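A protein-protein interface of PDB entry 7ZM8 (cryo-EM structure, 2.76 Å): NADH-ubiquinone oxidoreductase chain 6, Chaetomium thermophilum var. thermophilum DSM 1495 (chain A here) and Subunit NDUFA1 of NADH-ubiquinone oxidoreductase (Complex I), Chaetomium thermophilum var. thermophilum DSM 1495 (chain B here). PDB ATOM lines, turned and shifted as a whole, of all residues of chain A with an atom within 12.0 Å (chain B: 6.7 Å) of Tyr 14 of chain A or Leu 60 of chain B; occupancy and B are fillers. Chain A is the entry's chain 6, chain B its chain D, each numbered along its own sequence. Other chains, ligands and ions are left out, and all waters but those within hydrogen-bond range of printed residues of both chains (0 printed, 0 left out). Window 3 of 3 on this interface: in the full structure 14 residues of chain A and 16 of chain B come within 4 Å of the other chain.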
ATOM      1  N   LEU A  10      31.108   4.856 -17.727  1.00  0.00           N
ATOM      2  CA  LEU A  10      29.758   5.439 -17.482  1.00  0.00           C
ATOM      3  C   LEU A  10      28.770   4.893 -18.516  1.00  0.00           C
ATOM      4  O   LEU A  10      29.226   4.470 -19.581  1.00  0.00           O
ATOM      5  CB  LEU A  10      29.834   6.957 -17.656  1.00  0.00           C
ATOM      6  CG  LEU A  10      30.428   7.763 -16.510  1.00  0.00           C
ATOM      7  CD1 LEU A  10      31.876   8.123 -16.811  1.00  0.00           C
ATOM      8  CD2 LEU A  10      29.605   9.023 -16.302  1.00  0.00           C
ATOM      9  N   LYS A  11      27.471   4.919 -18.219  1.00  0.00           N
ATOM     10  CA  LYS A  11      26.450   4.498 -19.215  1.00  0.00           C
ATOM     11  C   LYS A  11      26.032   5.703 -20.060  1.00  0.00           C
ATOM     12  O   LYS A  11      25.712   6.739 -19.467  1.00  0.00           O
ATOM     13  CB  LYS A  11      25.220   3.902 -18.531  1.00  0.00           C
ATOM     14  CG  LYS A  11      24.248   3.188 -19.458  1.00  0.00           C
ATOM     15  CD  LYS A  11      23.111   2.507 -18.728  1.00  0.00           C
ATOM     16  CE  LYS A  11      22.207   1.716 -19.651  1.00  0.00           C
ATOM     17  NZ  LYS A  11      21.137   1.016 -18.903  1.00  0.00           N
ATOM     18  N   GLU A  12      26.056   5.571 -21.394  1.00  0.00           N
ATOM     19  CA  GLU A  12      25.571   6.656 -22.286  1.00  0.00           C
ATOM     20  C   GLU A  12      24.064   6.851 -22.101  1.00  0.00           C
ATOM     21  O   GLU A  12      23.382   5.865 -21.782  1.00  0.00           O
ATOM     22  CB  GLU A  12      25.912   6.328 -23.735  1.00  0.00           C
ATOM     23  CG  GLU A  12      27.309   5.776 -23.901  1.00  0.00           C
ATOM     24  CD  GLU A  12      27.630   5.367 -25.323  1.00  0.00           C
ATOM     25  OE1 GLU A  12      28.683   4.745 -25.538  1.00  0.00           O
ATOM     26  OE2 GLU A  12      26.825   5.679 -26.209  1.00  0.00           O
ATOM     27  N   ILE A  13      23.555   8.061 -22.338  1.00  0.00           N
ATOM     28  CA  ILE A  13      22.108   8.285 -22.059  1.00  0.00           C
ATOM     29  C   ILE A  13      21.252   8.476 -23.324  1.00  0.00           C
ATOM     30  O   ILE A  13      20.207   7.805 -23.404  1.00  0.00           O
ATOM     31  CB  ILE A  13      21.925   9.371 -20.976  1.00  0.00           C
ATOM     32  CG1 ILE A  13      20.451   9.617 -20.647  1.00  0.00           C
ATOM     33  CG2 ILE A  13      22.657  10.652 -21.346  1.00  0.00           C
ATOM     34  CD1 ILE A  13      20.232  10.530 -19.464  1.00  0.00           C
ATOM     35  N   TYR A  14      21.636   9.327 -24.277  1.00  0.00           N
ATOM     36  CA  TYR A  14      20.718   9.560 -25.432  1.00  0.00           C
ATOM     37  C   TYR A  14      21.335   9.095 -26.752  1.00  0.00           C
ATOM     38  O   TYR A  14      20.620   9.079 -27.767  1.00  0.00           O
ATOM     39  CB  TYR A  14      20.263  11.015 -25.483  1.00  0.00           C
ATOM     40  CG  TYR A  14      19.401  11.439 -24.323  1.00  0.00           C
ATOM     41  CD1 TYR A  14      18.088  11.011 -24.216  1.00  0.00           C
ATOM     42  CD2 TYR A  14      19.892  12.271 -23.332  1.00  0.00           C
ATOM     43  CE1 TYR A  14      17.287  11.393 -23.155  1.00  0.00           C
ATOM     44  CE2 TYR A  14      19.103  12.664 -22.264  1.00  0.00           C
ATOM     45  CZ  TYR A  14      17.796  12.225 -22.175  1.00  0.00           C
ATOM     46  OH  TYR A  14      17.015  12.612 -21.126  1.00  0.00           O
ATOM     47  N   THR A  15      22.610   8.711 -26.730  1.00  0.00           N
ATOM     48  CA  THR A  15      23.323   8.228 -27.935  1.00  0.00           C
ATOM     49  C   THR A  15      23.752   6.801 -27.607  1.00  0.00           C
ATOM     50  O   THR A  15      24.856   6.428 -28.010  1.00  0.00           O
ATOM     51  CB  THR A  15      24.502   9.165 -28.206  1.00  0.00           C
ATOM     52  OG1 THR A  15      25.269   9.232 -27.004  1.00  0.00           O
ATOM     53  CG2 THR A  15      24.066  10.560 -28.596  1.00  0.00           C
ATOM     54  N   ASN A  16      22.882   6.015 -26.974  1.00  0.00           N
ATOM     55  CA  ASN A  16      23.268   4.691 -26.418  1.00  0.00           C
ATOM     56  C   ASN A  16      23.157   3.515 -27.390  1.00  0.00           C
ATOM     57  O   ASN A  16      23.055   2.400 -26.887  1.00  0.00           O
ATOM     58  CB  ASN A  16      22.492   4.373 -25.141  1.00  0.00           C
ATOM     59  CG  ASN A  16      20.996   4.538 -25.304  1.00  0.00           C
ATOM     60  OD1 ASN A  16      20.511   5.632 -25.583  1.00  0.00           O
ATOM     61  ND2 ASN A  16      20.256   3.458 -25.117  1.00  0.00           N
ATOM     62  N   GLY A  17      23.049   3.724 -28.698  1.00  0.00           N
ATOM     63  CA  GLY A  17      23.103   2.586 -29.645  1.00  0.00           C
ATOM     64  C   GLY A  17      22.135   1.443 -29.371  1.00  0.00           C
ATOM     65  O   GLY A  17      21.025   1.721 -28.885  1.00  0.00           O
ATOM     66  N   SER A  18      22.520   0.204 -29.699  1.00  0.00           N
ATOM     67  CA  SER A  18      21.604  -0.957 -29.570  1.00  0.00           C
ATOM     68  C   SER A  18      22.263  -1.994 -28.673  1.00  0.00           C
ATOM     69  O   SER A  18      23.386  -1.768 -28.233  1.00  0.00           O
ATOM     70  CB  SER A  18      21.292  -1.563 -30.898  1.00  0.00           C
ATOM     71  OG  SER A  18      20.543  -0.664 -31.699  1.00  0.00           O
ATOM     72  N   LYS A 173      35.839  10.109 -32.259  1.00  0.00           N
ATOM     73  CA  LYS A 173      35.304  10.932 -33.375  1.00  0.00           C
ATOM     74  C   LYS A 173      36.422  11.509 -34.251  1.00  0.00           C
ATOM     75  O   LYS A 173      37.526  11.682 -33.731  1.00  0.00           O
ATOM     76  CB  LYS A 173      34.449  12.032 -32.738  1.00  0.00           C
ATOM     77  CG  LYS A 173      35.181  13.209 -32.120  1.00  0.00           C
ATOM     78  CD  LYS A 173      34.242  14.326 -31.725  1.00  0.00           C
ATOM     79  CE  LYS A 173      32.956  13.832 -31.097  1.00  0.00           C
ATOM     80  NZ  LYS A 173      32.213  14.912 -30.403  1.00  0.00           N
ATOM     81  N   TRP A 175      37.162  14.601 -37.628  1.00  0.00           N
ATOM     82  CA  TRP A 175      36.504  15.791 -38.225  1.00  0.00           C
ATOM     83  C   TRP A 175      36.816  15.906 -39.716  1.00  0.00           C
ATOM     84  O   TRP A 175      35.885  16.161 -40.493  1.00  0.00           O
ATOM     85  CB  TRP A 175      36.885  17.047 -37.442  1.00  0.00           C
ATOM     86  CG  TRP A 175      36.302  17.039 -36.064  1.00  0.00           C
ATOM     87  CD1 TRP A 175      36.942  16.732 -34.900  1.00  0.00           C
ATOM     88  CD2 TRP A 175      34.936  17.310 -35.712  1.00  0.00           C
ATOM     89  NE1 TRP A 175      36.075  16.820 -33.846  1.00  0.00           N
ATOM     90  CE2 TRP A 175      34.836  17.169 -34.312  1.00  0.00           C
ATOM     91  CE3 TRP A 175      33.793  17.667 -36.437  1.00  0.00           C
ATOM     92  CZ2 TRP A 175      33.642  17.377 -33.627  1.00  0.00           C
ATOM     93  CZ3 TRP A 175      32.614  17.872 -35.759  1.00  0.00           C
ATOM     94  CH2 TRP A 175      32.544  17.731 -34.374  1.00  0.00           C
ATOM     95  N   PHE B  32      11.181  18.023 -26.470  1.00  0.00           N
ATOM     96  CA  PHE B  32      12.265  17.014 -26.323  1.00  0.00           C
ATOM     97  C   PHE B  32      13.616  17.676 -26.556  1.00  0.00           C
ATOM     98  O   PHE B  32      14.597  17.257 -25.934  1.00  0.00           O
ATOM     99  CB  PHE B  32      12.056  15.816 -27.247  1.00  0.00           C
ATOM    100  CG  PHE B  32      12.913  14.615 -26.944  1.00  0.00           C
ATOM    101  CD1 PHE B  32      12.865  14.008 -25.704  1.00  0.00           C
ATOM    102  CD2 PHE B  32      13.756  14.084 -27.907  1.00  0.00           C
ATOM    103  CE1 PHE B  32      13.640  12.895 -25.431  1.00  0.00           C
ATOM    104  CE2 PHE B  32      14.532  12.970 -27.630  1.00  0.00           C
ATOM    105  CZ  PHE B  32      14.469  12.378 -26.393  1.00  0.00           C
ATOM    106  N   LYS B  47      26.033  14.977 -35.642  1.00  0.00           N
ATOM    107  CA  LYS B  47      25.948  14.143 -34.422  1.00  0.00           C
ATOM    108  C   LYS B  47      27.150  14.392 -33.516  1.00  0.00           C
ATOM    109  O   LYS B  47      26.977  14.366 -32.305  1.00  0.00           O
ATOM    110  CB  LYS B  47      25.866  12.682 -34.852  1.00  0.00           C
ATOM    111  CG  LYS B  47      24.618  12.286 -35.628  1.00  0.00           C
ATOM    112  CD  LYS B  47      24.665  10.845 -36.077  1.00  0.00           C
ATOM    113  CE  LYS B  47      23.410  10.379 -36.786  1.00  0.00           C
ATOM    114  NZ  LYS B  47      23.411  10.745 -38.221  1.00  0.00           N
ATOM    115  N   GLN B  49      28.964  17.204 -33.602  1.00  0.00           N
ATOM    116  CA  GLN B  49      28.815  18.619 -33.184  1.00  0.00           C
ATOM    117  C   GLN B  49      27.877  18.701 -31.975  1.00  0.00           C
ATOM    118  O   GLN B  49      28.142  19.519 -31.087  1.00  0.00           O
ATOM    119  CB  GLN B  49      28.418  19.494 -34.377  1.00  0.00           C
ATOM    120  CG  GLN B  49      29.576  19.859 -35.293  1.00  0.00           C
ATOM    121  CD  GLN B  49      30.463  20.967 -34.778  1.00  0.00           C
ATOM    122  OE1 GLN B  49      30.766  21.059 -33.593  1.00  0.00           O
ATOM    123  NE2 GLN B  49      30.908  21.821 -35.684  1.00  0.00           N
ATOM    124  N   MET B  50      26.827  17.885 -31.949  1.00  0.00           N
ATOM    125  CA  MET B  50      25.877  17.851 -30.805  1.00  0.00           C
ATOM    126  C   MET B  50      26.500  17.154 -29.598  1.00  0.00           C
ATOM    127  O   MET B  50      26.150  17.536 -28.478  1.00  0.00           O
ATOM    128  CB  MET B  50      24.591  17.123 -31.191  1.00  0.00           C
ATOM    129  CG  MET B  50      23.616  17.998 -31.949  1.00  0.00           C
ATOM    130  SD  MET B  50      22.050  17.166 -32.286  1.00  0.00           S
ATOM    131  CE  MET B  50      22.504  16.170 -33.704  1.00  0.00           C
ATOM    132  N   GLU B  51      27.366  16.165 -29.812  1.00  0.00           N
ATOM    133  CA  GLU B  51      28.076  15.500 -28.693  1.00  0.00           C
ATOM    134  C   GLU B  51      28.986  16.511 -28.005  1.00  0.00           C
ATOM    135  O   GLU B  51      29.163  16.404 -26.795  1.00  0.00           O
ATOM    136  CB  GLU B  51      28.706  14.203 -29.184  1.00  0.00           C
ATOM    137  CG  GLU B  51      27.698  13.089 -29.356  1.00  0.00           C
ATOM    138  CD  GLU B  51      28.304  11.710 -29.516  1.00  0.00           C
ATOM    139  OE1 GLU B  51      29.504  11.563 -29.229  1.00  0.00           O
ATOM    140  OE2 GLU B  51      27.572  10.788 -29.926  1.00  0.00           O
ATOM    141  N   ARG B  52      29.554  17.432 -28.769  1.00  0.00           N
ATOM    142  CA  ARG B  52      30.435  18.471 -28.206  1.00  0.00           C
ATOM    143  C   ARG B  52      29.560  19.530 -27.558  1.00  0.00           C
ATOM    144  O   ARG B  52      30.065  20.226 -26.678  1.00  0.00           O
ATOM    145  CB  ARG B  52      31.381  18.979 -29.286  1.00  0.00           C
ATOM    146  CG  ARG B  52      32.447  19.944 -28.794  1.00  0.00           C
ATOM    147  CD  ARG B  52      33.237  20.492 -29.960  1.00  0.00           C
ATOM    148  NE  ARG B  52      34.180  21.475 -29.467  1.00  0.00           N
ATOM    149  CZ  ARG B  52      34.001  22.779 -29.561  1.00  0.00           C
ATOM    150  NH1 ARG B  52      32.923  23.246 -30.164  1.00  0.00           N
ATOM    151  NH2 ARG B  52      34.902  23.608 -29.074  1.00  0.00           N
ATOM    152  N   ASP B  53      28.300  19.664 -27.988  1.00  0.00           N
ATOM    153  CA  ASP B  53      27.424  20.565 -27.247  1.00  0.00           C
ATOM    154  C   ASP B  53      27.140  20.022 -25.856  1.00  0.00           C
ATOM    155  O   ASP B  53      27.043  20.786 -24.892  1.00  0.00           O
ATOM    156  CB  ASP B  53      26.113  20.767 -28.003  1.00  0.00           C
ATOM    157  CG  ASP B  53      26.290  21.544 -29.281  1.00  0.00           C
ATOM    158  OD1 ASP B  53      27.215  22.373 -29.352  1.00  0.00           O
ATOM    159  OD2 ASP B  53      25.473  21.351 -30.207  1.00  0.00           O
ATOM    160  N   ARG B  54      26.986  18.706 -25.724  1.00  0.00           N
ATOM    161  CA  ARG B  54      26.811  18.067 -24.393  1.00  0.00           C
ATOM    162  C   ARG B  54      28.105  18.161 -23.589  1.00  0.00           C
ATOM    163  O   ARG B  54      28.022  18.191 -22.356  1.00  0.00           O
ATOM    164  CB  ARG B  54      26.367  16.613 -24.578  1.00  0.00           C
ATOM    165  CG  ARG B  54      25.896  15.930 -23.304  1.00  0.00           C
ATOM    166  CD  ARG B  54      25.071  14.688 -23.566  1.00  0.00           C
ATOM    167  NE  ARG B  54      25.795  13.742 -24.399  1.00  0.00           N
ATOM    168  CZ  ARG B  54      25.327  12.562 -24.781  1.00  0.00           C
ATOM    169  NH1 ARG B  54      26.066  11.776 -25.544  1.00  0.00           N
ATOM    170  NH2 ARG B  54      24.125  12.172 -24.401  1.00  0.00           N
ATOM    171  N   THR B  57      27.930  22.043 -22.419  1.00  0.00           N
ATOM    172  CA  THR B  57      26.760  22.447 -21.651  1.00  0.00           C
ATOM    173  C   THR B  57      26.079  21.322 -20.891  1.00  0.00           C
ATOM    174  O   THR B  57      25.426  21.594 -19.885  1.00  0.00           O
ATOM    175  CB  THR B  57      25.713  23.106 -22.564  1.00  0.00           C
ATOM    176  OG1 THR B  57      25.024  22.094 -23.304  1.00  0.00           O
ATOM    177  CG2 THR B  57      26.364  24.091 -23.522  1.00  0.00           C
ATOM    178  N   GLY B  58      26.204  20.076 -21.333  1.00  0.00           N
ATOM    179  CA  GLY B  58      25.483  18.971 -20.739  1.00  0.00           C
ATOM    180  C   GLY B  58      24.258  18.535 -21.511  1.00  0.00           C
ATOM    181  O   GLY B  58      23.744  17.443 -21.256  1.00  0.00           O
ATOM    182  N   HIS B  59      23.795  19.348 -22.453  1.00  0.00           N
ATOM    183  CA  HIS B  59      22.629  19.071 -23.276  1.00  0.00           C
ATOM    184  C   HIS B  59      23.059  18.989 -24.731  1.00  0.00           C
ATOM    185  O   HIS B  59      23.831  19.825 -25.201  1.00  0.00           O
ATOM    186  CB  HIS B  59      21.574  20.164 -23.088  1.00  0.00           C
ATOM    187  CG  HIS B  59      20.264  19.884 -23.759  1.00  0.00           C
ATOM    188  ND1 HIS B  59      19.997  18.687 -24.386  1.00  0.00           N
ATOM    189  CD2 HIS B  59      19.145  20.634 -23.893  1.00  0.00           C
ATOM    190  CE1 HIS B  59      18.774  18.714 -24.881  1.00  0.00           C
ATOM    191  NE2 HIS B  59      18.236  19.884 -24.597  1.00  0.00           N
ATOM    192  N   LEU B  60      22.555  17.976 -25.443  1.00  0.00           N
ATOM    193  CA  LEU B  60      22.947  17.778 -26.835  1.00  0.00           C
ATOM    194  C   LEU B  60      22.563  18.960 -27.712  1.00  0.00           C
ATOM    195  O   LEU B  60      23.169  19.167 -28.767  1.00  0.00           O
ATOM    196  CB  LEU B  60      22.327  16.494 -27.384  1.00  0.00           C
ATOM    197  CG  LEU B  60      22.920  15.180 -26.874  1.00  0.00           C
ATOM    198  CD1 LEU B  60      21.943  14.033 -27.039  1.00  0.00           C
ATOM    199  CD2 LEU B  60      24.237  14.869 -27.564  1.00  0.00           C
ATOM    200  N   ARG B  61      21.571  19.745 -27.305  1.00  0.00           N
ATOM    201  CA  ARG B  61      21.181  20.938 -28.037  1.00  0.00           C
ATOM    202  C   ARG B  61      21.599  22.223 -27.336  1.00  0.00           C
ATOM    203  O   ARG B  61      21.220  23.310 -27.781  1.00  0.00           O
ATOM    204  CB  ARG B  61      19.672  20.945 -28.279  1.00  0.00           C
ATOM    205  CG  ARG B  61      19.143  19.686 -28.929  1.00  0.00           C
ATOM    206  CD  ARG B  61      19.594  19.557 -30.372  1.00  0.00           C
ATOM    207  NE  ARG B  61      19.479  20.812 -31.104  1.00  0.00           N
ATOM    208  CZ  ARG B  61      18.373  21.226 -31.710  1.00  0.00           C
ATOM    209  NH1 ARG B  61      18.360  22.380 -32.350  1.00  0.00           N
ATOM    210  NH2 ARG B  61      17.280  20.485 -31.679  1.00  0.00           N
ATOM    211  N   GLY B  62      22.372  22.131 -26.258  1.00  0.00           N
ATOM    212  CA  GLY B  62      22.801  23.328 -25.567  1.00  0.00           C
ATOM    213  C   GLY B  62      23.820  24.116 -26.366  1.00  0.00           C
ATOM    214  O   GLY B  62      24.628  23.564 -27.108  1.00  0.00           O
ATOM    215  N   GLN B  63      23.786  25.435 -26.192  1.00  0.00           N
ATOM    216  CA  GLN B  63      24.607  26.354 -26.967  1.00  0.00           C
ATOM    217  C   GLN B  63      25.258  27.379 -26.056  1.00  0.00           C
ATOM    218  O   GLN B  63      24.650  27.836 -25.088  1.00  0.00           O
ATOM    219  CB  GLN B  63      23.777  27.073 -28.024  1.00  0.00           C
ATOM    220  CG  GLN B  63      23.094  26.160 -29.012  1.00  0.00           C
ATOM    221  CD  GLN B  63      24.056  25.580 -30.006  1.00  0.00           C
ATOM    222  OE1 GLN B  63      25.158  26.076 -30.174  1.00  0.00           O
ATOM    223  NE2 GLN B  63      23.644  24.518 -30.674  1.00  0.00           N
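NH1 of Arg 54 of chain B lies within hydrogen-bond range of OG1 of Thr 15 of chain A (3.0 Å).
O of Ile 13 of chain A sits close to OD1 of Asn 16 of chain A (3.1 Å).
The backbone carbonyl oxygen of His 59 of chain B sits at hydrogen-bond distance from the backbone NH of Arg 54 of chain B.
Among the printed residues, merely in contact across the chains: Trp 175 of chain A with Gln 49 of chain B, Ile 13 of chain A with Arg 54 of chain B, Thr 15 of chain A with Glu 51 of chain B, Lys 173 of chain A with Glu 51 of chain B, Tyr 14 of chain A with Arg 54 of chain B and Tyr 14 of chain A with Leu 60 of chain B.
Tyr 14 of chain A touches two residues of chain B.
Leu 60 of chain B touches just one residue of chain A: Tyr 14 (3.8 Å).
No residue of chain A comes within 4 Å of Met 50 of chain B.
Glu 51 of chain B touches just these residues of chain A: Thr 15 (3.8 Å) and Lys 173 (3.8 Å).
No residue of chain A comes within 4 Å of Asp 53 of chain B.
No residue of chain A comes within 4 Å of Thr 57 of chain B.
Arg 61 of chain B touches none of the printed residues of chain A.
Of the printed residues of chain A, Gln 49 of chain B touches Trp 175 (3.7 Å).
Of the printed residues of chain B, Trp 175 of chain A touches Gln 49.
Of the printed residues of chain B, Thr 15 of chain A touches Glu 51 (3.8 Å) and Arg 54 (3.0 Å).
Arg 52 of chain B touches none of the printed residues of chain A.
Glu 12 of chain A touches none of the printed residues of chain B.
The nearest residue of chain B that does not touch Tyr 14 of chain A is Phe 32 of chain B (4.4 Å).
The nearest residue of chain A that does not touch Leu 60 of chain B is Thr 15 of chain A (4.4 Å).
The nearest printed residue of chain A that does not touch Gln 49 of chain B is Lys 173 of chain A (5.1 Å).
Hydrophobic or aromatic side chains of chain A within 4 Å of the printed part of chain B: Ile 13, Tyr 14 and Trp 175.
Among the printed residues, no Asp or Glu carboxylate lies within 4 Å of a Lys or Arg side-chain nitrogen of the other chain.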
